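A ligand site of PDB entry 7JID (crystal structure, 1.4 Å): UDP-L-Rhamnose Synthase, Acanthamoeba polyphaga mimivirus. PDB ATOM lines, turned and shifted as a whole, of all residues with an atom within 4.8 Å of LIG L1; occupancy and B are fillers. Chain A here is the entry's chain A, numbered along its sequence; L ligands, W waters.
NE of Arg 61 is in salt-bridge range of OD2 of Asp 85 (2.7 Å).
An oxygen (O11) of LIG L1 lies close to the backbone carbonyl oxygen of Leu 107, 3.5 Å away.
Gly 10 touches LIG L1 (CA to O4, 3.8 Å).
Lys 12 touches LIG L1.
O of Phe 58 touches C11 of LIG L1, at 3.1 Å.
CA of Ile 59 touches O4 of LIG L1, at 3.3 Å.
Gly 60 touches LIG L1 (O to C6, 3.3 Å).
Thr 62 touches LIG L1.
Tyr 139 touches LIG L1 (OH to O12, 3.96 Å).
Lys 143 touches LIG L1 (NZ to O12, 3.9 Å).
Hydrophobic or aromatic side chains within 4 Å of LIG L1: Trp 14, Ile 15, Ala 37, Ile 59, His 63 and Leu 107.
The backbone NH of Ala 37 lies within hydrogen-bond range of a nitrogen (N4) of LIG L1 (3.0 Å).
The side-chain hydroxyl (OH) of Tyr 139 is in hydrogen-bond range of an oxygen (O8) of LG2 L2 (2.8 Å).
The side-chain carboxylate (OD1) of Asp 85 lies within hydrogen-bond range of a nitrogen (N3) of LIG L1 (2.9 Å).
O16 of LIG L1 lies within salt-bridge range of NH1 of Arg 61, 2.8 Å away.
The side-chain carboxylate (OD1) of Asp 38 is in hydrogen-bond range of a nitrogen (N3) of LIG L1 (3.0 Å).
O2 of LIG L1 is in hydrogen-bond range of NE2 of His 63, at 2.9 Å.
The backbone NH (N) of Gly 13 lies within hydrogen-bond range of an oxygen (O5) of LIG L1 (3.2 Å).
N of Ile 15 is in hydrogen-bond range of O9 of LIG L1.
The backbone NH (N) of Trp 14 is in hydrogen-bond range of an oxygen (O1) of LIG L1, at 2.8 Å.
The guanidinium group (NH2) of Arg 36 is in salt-bridge range of an oxygen (O16) of LIG L1.
Water W11 lies within hydrogen-bond range of O13 of LIG L1 (2.5 Å), O8 of LG2 L2 (2.6 Å) and O of Gly 108 (2.9 Å).
Water W12 lies within hydrogen-bond range of an oxygen (O2) of LIG L1 (2.7 Å) and the guanidinium group of Arg 61 (3.3 Å).
Water W10 lies within hydrogen-bond range of an oxygen (O9) of LIG L1 (2.7 Å), the backbone NH (N) of Gly 16 (2.8 Å), the backbone carbonyl oxygen (O) of Phe 58 (2.9 Å), the backbone carbonyl oxygen (O) of Gly 10 (3.3 Å) and the backbone NH (N) of Ile 15 (3.4 Å).
Water W8 lies within hydrogen-bond range of O2 of LIG L1 (2.7 Å), OG1 of Thr 62 (2.8 Å) and O of Gly 60 (2.8 Å).
Water W4 lies within hydrogen-bond range of N5 of LIG L1 and N of Gly 10.
Water W2 bridges O5 of LIG L1 (2.8 Å) and N of Lys 12 (3.2 Å).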
ATOM      1  N   GLY A  10       0.591  -1.563 -21.126  1.00  0.00           N
ATOM      2  CA  GLY A  10       0.610  -3.021 -20.910  1.00  0.00           C
ATOM      3  C   GLY A  10      -0.668  -3.509 -20.241  1.00  0.00           C
ATOM      4  O   GLY A  10      -0.673  -4.596 -19.614  1.00  0.00           O
ATOM      5  N   LYS A  12      -3.297  -4.880 -21.311  1.00  0.00           N
ATOM      6  CA  LYS A  12      -3.809  -6.148 -21.885  1.00  0.00           C
ATOM      7  C   LYS A  12      -2.861  -7.287 -21.539  1.00  0.00           C
ATOM      8  O   LYS A  12      -3.173  -8.431 -21.854  1.00  0.00           O
ATOM      9  CB  LYS A  12      -3.924  -6.064 -23.411  1.00  0.00           C
ATOM     10  CG  LYS A  12      -4.815  -4.942 -23.902  1.00  0.00           C
ATOM     11  CD  LYS A  12      -6.149  -4.892 -23.201  1.00  0.00           C
ATOM     12  CE  LYS A  12      -7.317  -4.864 -24.161  1.00  0.00           C
ATOM     13  NZ  LYS A  12      -7.587  -6.213 -24.719  1.00  0.00           N
ATOM     14  N   GLY A  13      -1.720  -6.983 -20.948  1.00  0.00           N
ATOM     15  CA  GLY A  13      -0.771  -8.050 -20.615  1.00  0.00           C
ATOM     16  C   GLY A  13      -1.210  -8.829 -19.392  1.00  0.00           C
ATOM     17  O   GLY A  13      -2.199  -8.445 -18.716  1.00  0.00           O
ATOM     18  N   TRP A  14      -0.444  -9.864 -19.036  1.00  0.00           N
ATOM     19  CA  TRP A  14      -0.802 -10.708 -17.863  1.00  0.00           C
ATOM     20  C   TRP A  14      -0.859  -9.846 -16.607  1.00  0.00           C
ATOM     21  O   TRP A  14      -1.896  -9.848 -15.909  1.00  0.00           O
ATOM     22  CB  TRP A  14       0.183 -11.863 -17.784  1.00  0.00           C
ATOM     23  CG  TRP A  14       0.029 -12.746 -16.599  1.00  0.00           C
ATOM     24  CD1 TRP A  14      -1.085 -13.404 -16.199  1.00  0.00           C
ATOM     25  CD2 TRP A  14       1.076 -13.125 -15.692  1.00  0.00           C
ATOM     26  NE1 TRP A  14      -0.819 -14.144 -15.076  1.00  0.00           N
ATOM     27  CE2 TRP A  14       0.508 -13.992 -14.739  1.00  0.00           C
ATOM     28  CE3 TRP A  14       2.431 -12.782 -15.564  1.00  0.00           C
ATOM     29  CZ2 TRP A  14       1.241 -14.540 -13.696  1.00  0.00           C
ATOM     30  CZ3 TRP A  14       3.166 -13.319 -14.538  1.00  0.00           C
ATOM     31  CH2 TRP A  14       2.590 -14.208 -13.625  1.00  0.00           C
ATOM     32  N   ILE A  15       0.255  -9.205 -16.226  1.00  0.00           N
ATOM     33  CA  ILE A  15       0.320  -8.397 -14.994  1.00  0.00           C
ATOM     34  C   ILE A  15      -0.540  -7.153 -15.150  1.00  0.00           C
ATOM     35  O   ILE A  15      -1.228  -6.814 -14.221  1.00  0.00           O
ATOM     36  CB  ILE A  15       1.755  -8.113 -14.567  1.00  0.00           C
ATOM     37  CG1 ILE A  15       2.498  -9.439 -14.388  1.00  0.00           C
ATOM     38  CG2 ILE A  15       1.771  -7.229 -13.343  1.00  0.00           C
ATOM     39  CD1 ILE A  15       3.930  -9.256 -13.917  1.00  0.00           C
ATOM     40  N   GLY A  16      -0.454  -6.453 -16.284  1.00  0.00           N
ATOM     41  CA  GLY A  16      -1.221  -5.203 -16.419  1.00  0.00           C
ATOM     42  C   GLY A  16      -2.705  -5.426 -16.290  1.00  0.00           C
ATOM     43  O   GLY A  16      -3.363  -4.571 -15.650  1.00  0.00           O
ATOM     44  N   SER A  35      -1.257   4.434 -26.902  1.00  0.00           N
ATOM     45  CA  SER A  35       0.055   4.711 -27.544  1.00  0.00           C
ATOM     46  C   SER A  35       1.038   3.570 -27.228  1.00  0.00           C
ATOM     47  O   SER A  35       0.896   2.954 -26.171  1.00  0.00           O
ATOM     48  CB  SER A  35       0.618   6.058 -27.162  1.00  0.00           C
ATOM     49  OG  SER A  35       0.935   6.120 -25.783  1.00  0.00           O
ATOM     50  N   ARG A  36       1.931   3.284 -28.171  1.00  0.00           N
ATOM     51  CA  ARG A  36       3.111   2.403 -27.955  1.00  0.00           C
ATOM     52  C   ARG A  36       4.147   3.212 -27.181  1.00  0.00           C
ATOM     53  O   ARG A  36       4.367   4.395 -27.504  1.00  0.00           O
ATOM     54  CB  ARG A  36       3.612   1.839 -29.276  1.00  0.00           C
ATOM     55  CG  ARG A  36       2.574   1.072 -30.083  1.00  0.00           C
ATOM     56  CD  ARG A  36       1.957  -0.034 -29.291  1.00  0.00           C
ATOM     57  NE  ARG A  36       2.936  -1.094 -29.009  1.00  0.00           N
ATOM     58  CZ  ARG A  36       2.580  -2.294 -28.565  1.00  0.00           C
ATOM     59  NH1 ARG A  36       1.314  -2.551 -28.298  1.00  0.00           N
ATOM     60  NH2 ARG A  36       3.466  -3.242 -28.408  1.00  0.00           N
ATOM     61  N   ALA A  37       4.750   2.616 -26.169  1.00  0.00           N
ATOM     62  CA  ALA A  37       5.633   3.354 -25.240  1.00  0.00           C
ATOM     63  C   ALA A  37       6.844   3.918 -25.982  1.00  0.00           C
ATOM     64  O   ALA A  37       7.366   4.897 -25.529  1.00  0.00           O
ATOM     65  CB  ALA A  37       6.036   2.507 -24.076  1.00  0.00           C
ATOM     66  N   ASP A  38       7.278   3.216 -27.020  1.00  0.00           N
ATOM     67  CA  ASP A  38       8.418   3.599 -27.865  1.00  0.00           C
ATOM     68  C   ASP A  38       8.055   4.681 -28.897  1.00  0.00           C
ATOM     69  O   ASP A  38       8.944   5.130 -29.614  1.00  0.00           O
ATOM     70  CB  ASP A  38       8.994   2.332 -28.518  1.00  0.00           C
ATOM     71  CG  ASP A  38       7.951   1.596 -29.366  1.00  0.00           C
ATOM     72  OD1 ASP A  38       7.021   1.041 -28.760  1.00  0.00           O
ATOM     73  OD2 ASP A  38       8.077   1.657 -30.599  1.00  0.00           O
ATOM     74  N   PHE A  58       3.588  -1.843 -17.406  1.00  0.00           N
ATOM     75  CA  PHE A  58       3.639  -3.322 -17.354  1.00  0.00           C
ATOM     76  C   PHE A  58       4.029  -3.879 -18.692  1.00  0.00           C
ATOM     77  O   PHE A  58       3.397  -4.833 -19.149  1.00  0.00           O
ATOM     78  CB  PHE A  58       2.326  -3.877 -16.817  1.00  0.00           C
ATOM     79  CG  PHE A  58       1.950  -3.276 -15.497  1.00  0.00           C
ATOM     80  CD1 PHE A  58       2.752  -3.474 -14.387  1.00  0.00           C
ATOM     81  CD2 PHE A  58       0.856  -2.419 -15.378  1.00  0.00           C
ATOM     82  CE1 PHE A  58       2.461  -2.875 -13.161  1.00  0.00           C
ATOM     83  CE2 PHE A  58       0.554  -1.853 -14.151  1.00  0.00           C
ATOM     84  CZ  PHE A  58       1.364  -2.048 -13.061  1.00  0.00           C
ATOM     85  N   ILE A  59       5.026  -3.257 -19.327  1.00  0.00           N
ATOM     86  CA  ILE A  59       5.382  -3.603 -20.717  1.00  0.00           C
ATOM     87  C   ILE A  59       6.716  -4.341 -20.693  1.00  0.00           C
ATOM     88  O   ILE A  59       7.575  -4.127 -19.815  1.00  0.00           O
ATOM     89  CB  ILE A  59       5.454  -2.391 -21.672  1.00  0.00           C
ATOM     90  CG1 ILE A  59       6.650  -1.505 -21.348  1.00  0.00           C
ATOM     91  CG2 ILE A  59       4.113  -1.655 -21.675  1.00  0.00           C
ATOM     92  CD1 ILE A  59       6.828  -0.316 -22.263  1.00  0.00           C
ATOM     93  N   GLY A  60       6.928  -5.073 -21.779  1.00  0.00           N
ATOM     94  CA  GLY A  60       8.230  -5.673 -22.104  1.00  0.00           C
ATOM     95  C   GLY A  60       8.080  -6.773 -23.118  1.00  0.00           C
ATOM     96  O   GLY A  60       6.943  -7.085 -23.521  1.00  0.00           O
ATOM     97  N   ARG A  61       9.198  -7.337 -23.502  1.00  0.00           N
ATOM     98  CA  ARG A  61       9.235  -8.392 -24.536  1.00  0.00           C
ATOM     99  C   ARG A  61       9.960  -9.574 -23.922  1.00  0.00           C
ATOM    100  O   ARG A  61      11.146  -9.455 -23.656  1.00  0.00           O
ATOM    101  CB  ARG A  61       9.845  -7.869 -25.832  1.00  0.00           C
ATOM    102  CG  ARG A  61       9.695  -8.822 -27.004  1.00  0.00           C
ATOM    103  CD  ARG A  61       8.281  -8.970 -27.521  1.00  0.00           C
ATOM    104  NE  ARG A  61       7.579  -7.695 -27.533  1.00  0.00           N
ATOM    105  CZ  ARG A  61       6.275  -7.523 -27.587  1.00  0.00           C
ATOM    106  NH1 ARG A  61       5.761  -6.296 -27.512  1.00  0.00           N
ATOM    107  NH2 ARG A  61       5.455  -8.559 -27.687  1.00  0.00           N
ATOM    108  N   THR A  62       9.199 -10.616 -23.583  1.00  0.00           N
ATOM    109  CA  THR A  62       9.688 -11.690 -22.667  1.00  0.00           C
ATOM    110  C   THR A  62       9.351 -13.082 -23.193  1.00  0.00           C
ATOM    111  O   THR A  62       9.690 -14.051 -22.476  1.00  0.00           O
ATOM    112  CB  THR A  62       9.120 -11.528 -21.264  1.00  0.00           C
ATOM    113  OG1 THR A  62       7.690 -11.661 -21.320  1.00  0.00           O
ATOM    114  CG2 THR A  62       9.588 -10.220 -20.648  1.00  0.00           C
ATOM    115  N   HIS A  63       8.731 -13.137 -24.346  1.00  0.00           N
ATOM    116  CA  HIS A  63       8.266 -14.387 -25.021  1.00  0.00           C
ATOM    117  C   HIS A  63       7.720 -13.962 -26.371  1.00  0.00           C
ATOM    118  O   HIS A  63       7.382 -12.762 -26.557  1.00  0.00           O
ATOM    119  CB  HIS A  63       7.168 -15.104 -24.224  1.00  0.00           C
ATOM    120  CG  HIS A  63       5.951 -14.268 -24.009  1.00  0.00           C
ATOM    121  ND1 HIS A  63       4.801 -14.404 -24.783  1.00  0.00           N
ATOM    122  CD2 HIS A  63       5.707 -13.277 -23.136  1.00  0.00           C
ATOM    123  CE1 HIS A  63       3.909 -13.509 -24.387  1.00  0.00           C
ATOM    124  NE2 HIS A  63       4.461 -12.783 -23.395  1.00  0.00           N
ATOM    125  N   LYS A  84      13.775  -2.049 -27.824  1.00  0.00           N
ATOM    126  CA  LYS A  84      12.566  -1.212 -28.014  1.00  0.00           C
ATOM    127  C   LYS A  84      11.658  -1.373 -26.771  1.00  0.00           C
ATOM    128  O   LYS A  84      11.164  -0.338 -26.215  1.00  0.00           O
ATOM    129  CB  LYS A  84      11.789  -1.674 -29.251  1.00  0.00           C
ATOM    130  CG  LYS A  84      10.501  -0.886 -29.511  1.00  0.00           C
ATOM    131  CD  LYS A  84       9.530  -1.553 -30.457  1.00  0.00           C
ATOM    132  CE  LYS A  84      10.127  -1.899 -31.792  1.00  0.00           C
ATOM    133  NZ  LYS A  84       9.181  -2.827 -32.456  1.00  0.00           N
ATOM    134  N   ASP A  85      11.321  -2.600 -26.401  1.00  0.00           N
ATOM    135  CA  ASP A  85      10.256  -2.845 -25.419  1.00  0.00           C
ATOM    136  C   ASP A  85      10.823  -2.843 -24.008  1.00  0.00           C
ATOM    137  O   ASP A  85      10.050  -2.573 -23.090  1.00  0.00           O
ATOM    138  CB  ASP A  85       9.494  -4.124 -25.769  1.00  0.00           C
ATOM    139  CG  ASP A  85       8.762  -4.068 -27.113  1.00  0.00           C
ATOM    140  OD1 ASP A  85       8.424  -2.951 -27.578  1.00  0.00           O
ATOM    141  OD2 ASP A  85       8.509  -5.167 -27.689  1.00  0.00           O
ATOM    142  N   LEU A 107       7.356  -1.438 -13.700  1.00  0.00           N
ATOM    143  CA  LEU A 107       7.562  -2.839 -13.211  1.00  0.00           C
ATOM    144  C   LEU A 107       8.764  -3.425 -13.941  1.00  0.00           C
ATOM    145  O   LEU A 107       8.657  -3.675 -15.162  1.00  0.00           O
ATOM    146  CB  LEU A 107       6.318  -3.681 -13.431  1.00  0.00           C
ATOM    147  CG  LEU A 107       6.306  -4.985 -12.620  1.00  0.00           C
ATOM    148  CD1 LEU A 107       6.541  -4.758 -11.139  1.00  0.00           C
ATOM    149  CD2 LEU A 107       4.992  -5.729 -12.815  1.00  0.00           C
ATOM    150  N   GLY A 108       9.907  -3.454 -13.249  1.00  0.00           N
ATOM    151  CA  GLY A 108      11.162  -3.990 -13.795  1.00  0.00           C
ATOM    152  C   GLY A 108      11.397  -5.414 -13.326  1.00  0.00           C
ATOM    153  O   GLY A 108      10.473  -6.211 -13.173  1.00  0.00           O
ATOM    154  N   TYR A 139      17.939 -10.663 -22.417  1.00  0.00           N
ATOM    155  CA  TYR A 139      16.886 -10.026 -21.568  1.00  0.00           C
ATOM    156  C   TYR A 139      17.545  -9.384 -20.346  1.00  0.00           C
ATOM    157  O   TYR A 139      17.341  -8.194 -20.022  1.00  0.00           O
ATOM    158  CB  TYR A 139      15.888 -11.055 -21.059  1.00  0.00           C
ATOM    159  CG  TYR A 139      14.880 -10.496 -20.083  1.00  0.00           C
ATOM    160  CD1 TYR A 139      13.784  -9.742 -20.522  1.00  0.00           C
ATOM    161  CD2 TYR A 139      14.974 -10.780 -18.737  1.00  0.00           C
ATOM    162  CE1 TYR A 139      12.864  -9.246 -19.618  1.00  0.00           C
ATOM    163  CE2 TYR A 139      14.037 -10.290 -17.816  1.00  0.00           C
ATOM    164  CZ  TYR A 139      12.973  -9.548 -18.268  1.00  0.00           C
ATOM    165  OH  TYR A 139      12.055  -9.071 -17.352  1.00  0.00           O
ATOM    166  N   LYS A 143      17.726  -5.385 -19.510  1.00  0.00           N
ATOM    167  CA  LYS A 143      16.980  -5.004 -18.288  1.00  0.00           C
ATOM    168  C   LYS A 143      17.924  -4.452 -17.228  1.00  0.00           C
ATOM    169  O   LYS A 143      17.494  -3.573 -16.496  1.00  0.00           O
ATOM    170  CB  LYS A 143      16.098  -6.133 -17.775  1.00  0.00           C
ATOM    171  CG  LYS A 143      14.841  -6.357 -18.599  1.00  0.00           C
ATOM    172  CD  LYS A 143      13.764  -5.268 -18.342  1.00  0.00           C
ATOM    173  CE  LYS A 143      12.415  -5.549 -18.897  1.00  0.00           C
ATOM    174  NZ  LYS A 143      11.419  -4.549 -18.453  1.00  0.00           N
ATOM    175  N   ILE A 162      10.660  -7.172  -9.639  1.00  0.00           N
ATOM    176  CA  ILE A 162      10.013  -8.467  -9.344  1.00  0.00           C
ATOM    177  C   ILE A 162      10.902  -9.570  -9.932  1.00  0.00           C
ATOM    178  O   ILE A 162      11.688  -9.295 -10.849  1.00  0.00           O
ATOM    179  CB  ILE A 162       8.570  -8.544  -9.857  1.00  0.00           C
ATOM    180  CG1 ILE A 162       8.505  -8.336 -11.367  1.00  0.00           C
ATOM    181  CG2 ILE A 162       7.699  -7.587  -9.071  1.00  0.00           C
ATOM    182  CD1 ILE A 162       7.231  -8.919 -11.967  1.00  0.00           C
ATOM    183  N   ARG A 173       2.312 -17.771 -17.964  1.00  0.00           N
ATOM    184  CA  ARG A 173       3.355 -16.822 -17.496  1.00  0.00           C
ATOM    185  C   ARG A 173       3.766 -17.106 -16.033  1.00  0.00           C
ATOM    186  O   ARG A 173       4.880 -16.666 -15.635  1.00  0.00           O
ATOM    187  CB  ARG A 173       2.855 -15.382 -17.618  1.00  0.00           C
ATOM    188  CG  ARG A 173       2.553 -14.889 -19.038  1.00  0.00           C
ATOM    189  CD  ARG A 173       3.769 -14.439 -19.850  1.00  0.00           C
ATOM    190  NE  ARG A 173       4.478 -15.561 -20.459  1.00  0.00           N
ATOM    191  CZ  ARG A 173       4.045 -16.285 -21.489  1.00  0.00           C
ATOM    192  NH1 ARG A 173       2.884 -16.014 -22.054  1.00  0.00           N
ATOM    193  NH2 ARG A 173       4.781 -17.278 -21.974  1.00  0.00           N
HETATM  194  P1  LIG L   1       2.968  -9.889 -21.024  1.00  0.00           P
HETATM  195  O1  LIG L   1       1.718 -10.673 -20.705  1.00  0.00           O
HETATM  196  O2  LIG L   1       3.729 -10.221 -22.271  1.00  0.00           O
HETATM  197  O3  LIG L   1       2.454  -8.390 -21.028  1.00  0.00           O
HETATM  198  C1  LIG L   1       3.251  -7.351 -21.614  1.00  0.00           C
HETATM  199  C2  LIG L   1       2.439  -6.244 -22.255  1.00  0.00           C
HETATM  200  O4  LIG L   1       3.276  -5.170 -22.668  1.00  0.00           O
HETATM  201  C3  LIG L   1       1.732  -6.809 -23.485  1.00  0.00           C
HETATM  202  O5  LIG L   1       0.368  -6.376 -23.301  1.00  0.00           O
HETATM  203  C4  LIG L   1       2.428  -6.072 -24.629  1.00  0.00           C
HETATM  204  O6  LIG L   1       1.473  -5.726 -25.588  1.00  0.00           O
HETATM  205  C5  LIG L   1       2.950  -4.781 -23.990  1.00  0.00           C
HETATM  206  N1  LIG L   1       4.045  -4.089 -24.623  1.00  0.00           N
HETATM  207  C6  LIG L   1       5.252  -4.557 -24.894  1.00  0.00           C
HETATM  208  N2  LIG L   1       6.014  -3.621 -25.444  1.00  0.00           N
HETATM  209  C7  LIG L   1       5.270  -2.505 -25.541  1.00  0.00           C
HETATM  210  C8  LIG L   1       5.497  -1.215 -26.058  1.00  0.00           C
HETATM  211  N3  LIG L   1       6.669  -0.923 -26.572  1.00  0.00           N
HETATM  212  N4  LIG L   1       4.431  -0.333 -26.002  1.00  0.00           N
HETATM  213  C9  LIG L   1       3.272  -0.701 -25.451  1.00  0.00           C
HETATM  214  N5  LIG L   1       2.961  -1.908 -24.944  1.00  0.00           N
HETATM  215  C10 LIG L   1       3.972  -2.820 -24.980  1.00  0.00           C
HETATM  216  O7  LIG L   1       4.088  -9.881 -19.870  1.00  0.00           O
HETATM  217  P2  LIG L   1       3.850  -9.715 -18.273  1.00  0.00           P
HETATM  218  O8  LIG L   1       4.500 -10.998 -17.772  1.00  0.00           O
HETATM  219  O9  LIG L   1       2.540  -9.195 -17.856  1.00  0.00           O
HETATM  220  O10 LIG L   1       4.966  -8.643 -17.954  1.00  0.00           O
HETATM  221  C11 LIG L   1       4.887  -7.221 -17.832  1.00  0.00           C
HETATM  222  C12 LIG L   1       6.323  -6.653 -17.990  1.00  0.00           C
HETATM  223  O11 LIG L   1       6.629  -5.966 -16.815  1.00  0.00           O
HETATM  224  C13 LIG L   1       7.310  -7.808 -18.078  1.00  0.00           C
HETATM  225  O12 LIG L   1       8.658  -7.364 -18.463  1.00  0.00           O
HETATM  226  C14 LIG L   1       7.043  -8.259 -16.628  1.00  0.00           C
HETATM  227  O13 LIG L   1       7.969  -9.162 -16.003  1.00  0.00           O
HETATM  228  C15 LIG L   1       7.017  -6.967 -15.860  1.00  0.00           C
HETATM  229  P3  LIG L   1       1.596  -6.216 -27.088  1.00  0.00           P
HETATM  230  O14 LIG L   1       1.168  -7.617 -27.168  1.00  0.00           O
HETATM  231  O15 LIG L   1       0.520  -5.278 -27.657  1.00  0.00           O
HETATM  232  O16 LIG L   1       2.987  -5.996 -27.703  1.00  0.00           O
HETATM  233  P1  LG2 L   2      11.659 -19.735 -17.738  1.00  0.00           P
HETATM  234  O1  LG2 L   2      12.634 -19.939 -18.842  1.00  0.00           O
HETATM  235  O2  LG2 L   2      10.292 -20.403 -17.846  1.00  0.00           O
HETATM  236  O3  LG2 L   2      11.157 -18.212 -17.436  1.00  0.00           O
HETATM  237  P2  LG2 L   2      11.962 -16.821 -17.809  1.00  0.00           P
HETATM  238  O4  LG2 L   2      13.439 -16.769 -17.329  1.00  0.00           O
HETATM  239  O5  LG2 L   2      11.641 -16.469 -19.274  1.00  0.00           O
HETATM  240  O6  LG2 L   2      11.150 -15.864 -16.809  1.00  0.00           O
HETATM  241  C1  LG2 L   2      10.935 -12.245 -16.766  1.00  0.00           C
HETATM  242  O7  LG2 L   2      10.617 -13.624 -16.909  1.00  0.00           O
HETATM  243  C2  LG2 L   2      11.078 -11.913 -15.295  1.00  0.00           C
HETATM  244  O8  LG2 L   2      11.571 -10.573 -15.098  1.00  0.00           O
HETATM  245  C3  LG2 L   2      12.047 -12.862 -14.680  1.00  0.00           C
HETATM  246  O9  LG2 L   2      11.953 -12.738 -13.276  1.00  0.00           O
HETATM  247  C4  LG2 L   2      11.731 -14.332 -14.964  1.00  0.00           C
HETATM  248  C5  LG2 L   2      11.461 -14.558 -16.391  1.00  0.00           C
HETATM  249  N1  LG2 L   2      13.539 -24.147 -15.731  1.00  0.00           N
HETATM  250  C6  LG2 L   2      13.672 -25.480 -15.403  1.00  0.00           C
HETATM  251  O10 LG2 L   2      13.756 -25.821 -14.202  1.00  0.00           O
HETATM  252  N2  LG2 L   2      13.581 -26.411 -16.406  1.00  0.00           N
HETATM  253  C7  LG2 L   2      13.505 -26.059 -17.718  1.00  0.00           C
HETATM  254  O11 LG2 L   2      13.402 -26.993 -18.582  1.00  0.00           O
HETATM  255  C8  LG2 L   2      13.345 -24.716 -18.045  1.00  0.00           C
HETATM  256  C9  LG2 L   2      13.468 -23.735 -17.052  1.00  0.00           C
HETATM  257  C10 LG2 L   2      13.608 -23.091 -14.676  1.00  0.00           C
HETATM  258  C11 LG2 L   2      14.551 -21.919 -14.935  1.00  0.00           C
HETATM  259  C12 LG2 L   2      13.867 -20.787 -14.124  1.00  0.00           C
HETATM  260  C13 LG2 L   2      12.428 -21.157 -14.248  1.00  0.00           C
HETATM  261  C14 LG2 L   2      11.601 -20.285 -15.162  1.00  0.00           C
HETATM  262  C15 LG2 L   2       9.769 -11.518 -17.426  1.00  0.00           C
HETATM  263  O12 LG2 L   2      10.500 -14.631 -14.333  1.00  0.00           O
HETATM  264  O13 LG2 L   2      15.813 -22.239 -14.431  1.00  0.00           O
HETATM  265  O14 LG2 L   2      14.193 -20.893 -12.754  1.00  0.00           O
HETATM  266  O15 LG2 L   2      12.343 -22.470 -14.786  1.00  0.00           O
HETATM  267  O16 LG2 L   2      12.342 -20.196 -16.409  1.00  0.00           O
HETATM  268  O   HOH W   1      -0.465  -8.730 -29.009  1.00  0.00           O
HETATM  269  O   HOH W   2      -1.089  -4.009 -23.474  1.00  0.00           O
HETATM  270  O   HOH W   3      -0.837  -7.860 -25.120  1.00  0.00           O
HETATM  271  O   HOH W   4       0.422  -1.633 -23.922  1.00  0.00           O
HETATM  272  O   HOH W   5       6.372 -11.480 -15.786  1.00  0.00           O
HETATM  273  O   HOH W   6       3.593  -6.487 -30.326  1.00  0.00           O
HETATM  274  O   HOH W   7      -2.074  -4.780 -26.347  1.00  0.00           O
HETATM  275  O   HOH W   8       6.316  -9.384 -22.075  1.00  0.00           O
HETATM  276  O   HOH W   9       6.219 -12.514 -18.988  1.00  0.00           O
HETATM  277  O   HOH W  10       1.416  -6.843 -18.399  1.00  0.00           O
HETATM  278  O   HOH W  11       9.838  -8.759 -14.390  1.00  0.00           O
HETATM  279  O   HOH W  12       4.372  -9.289 -24.667  1.00  0.00           O
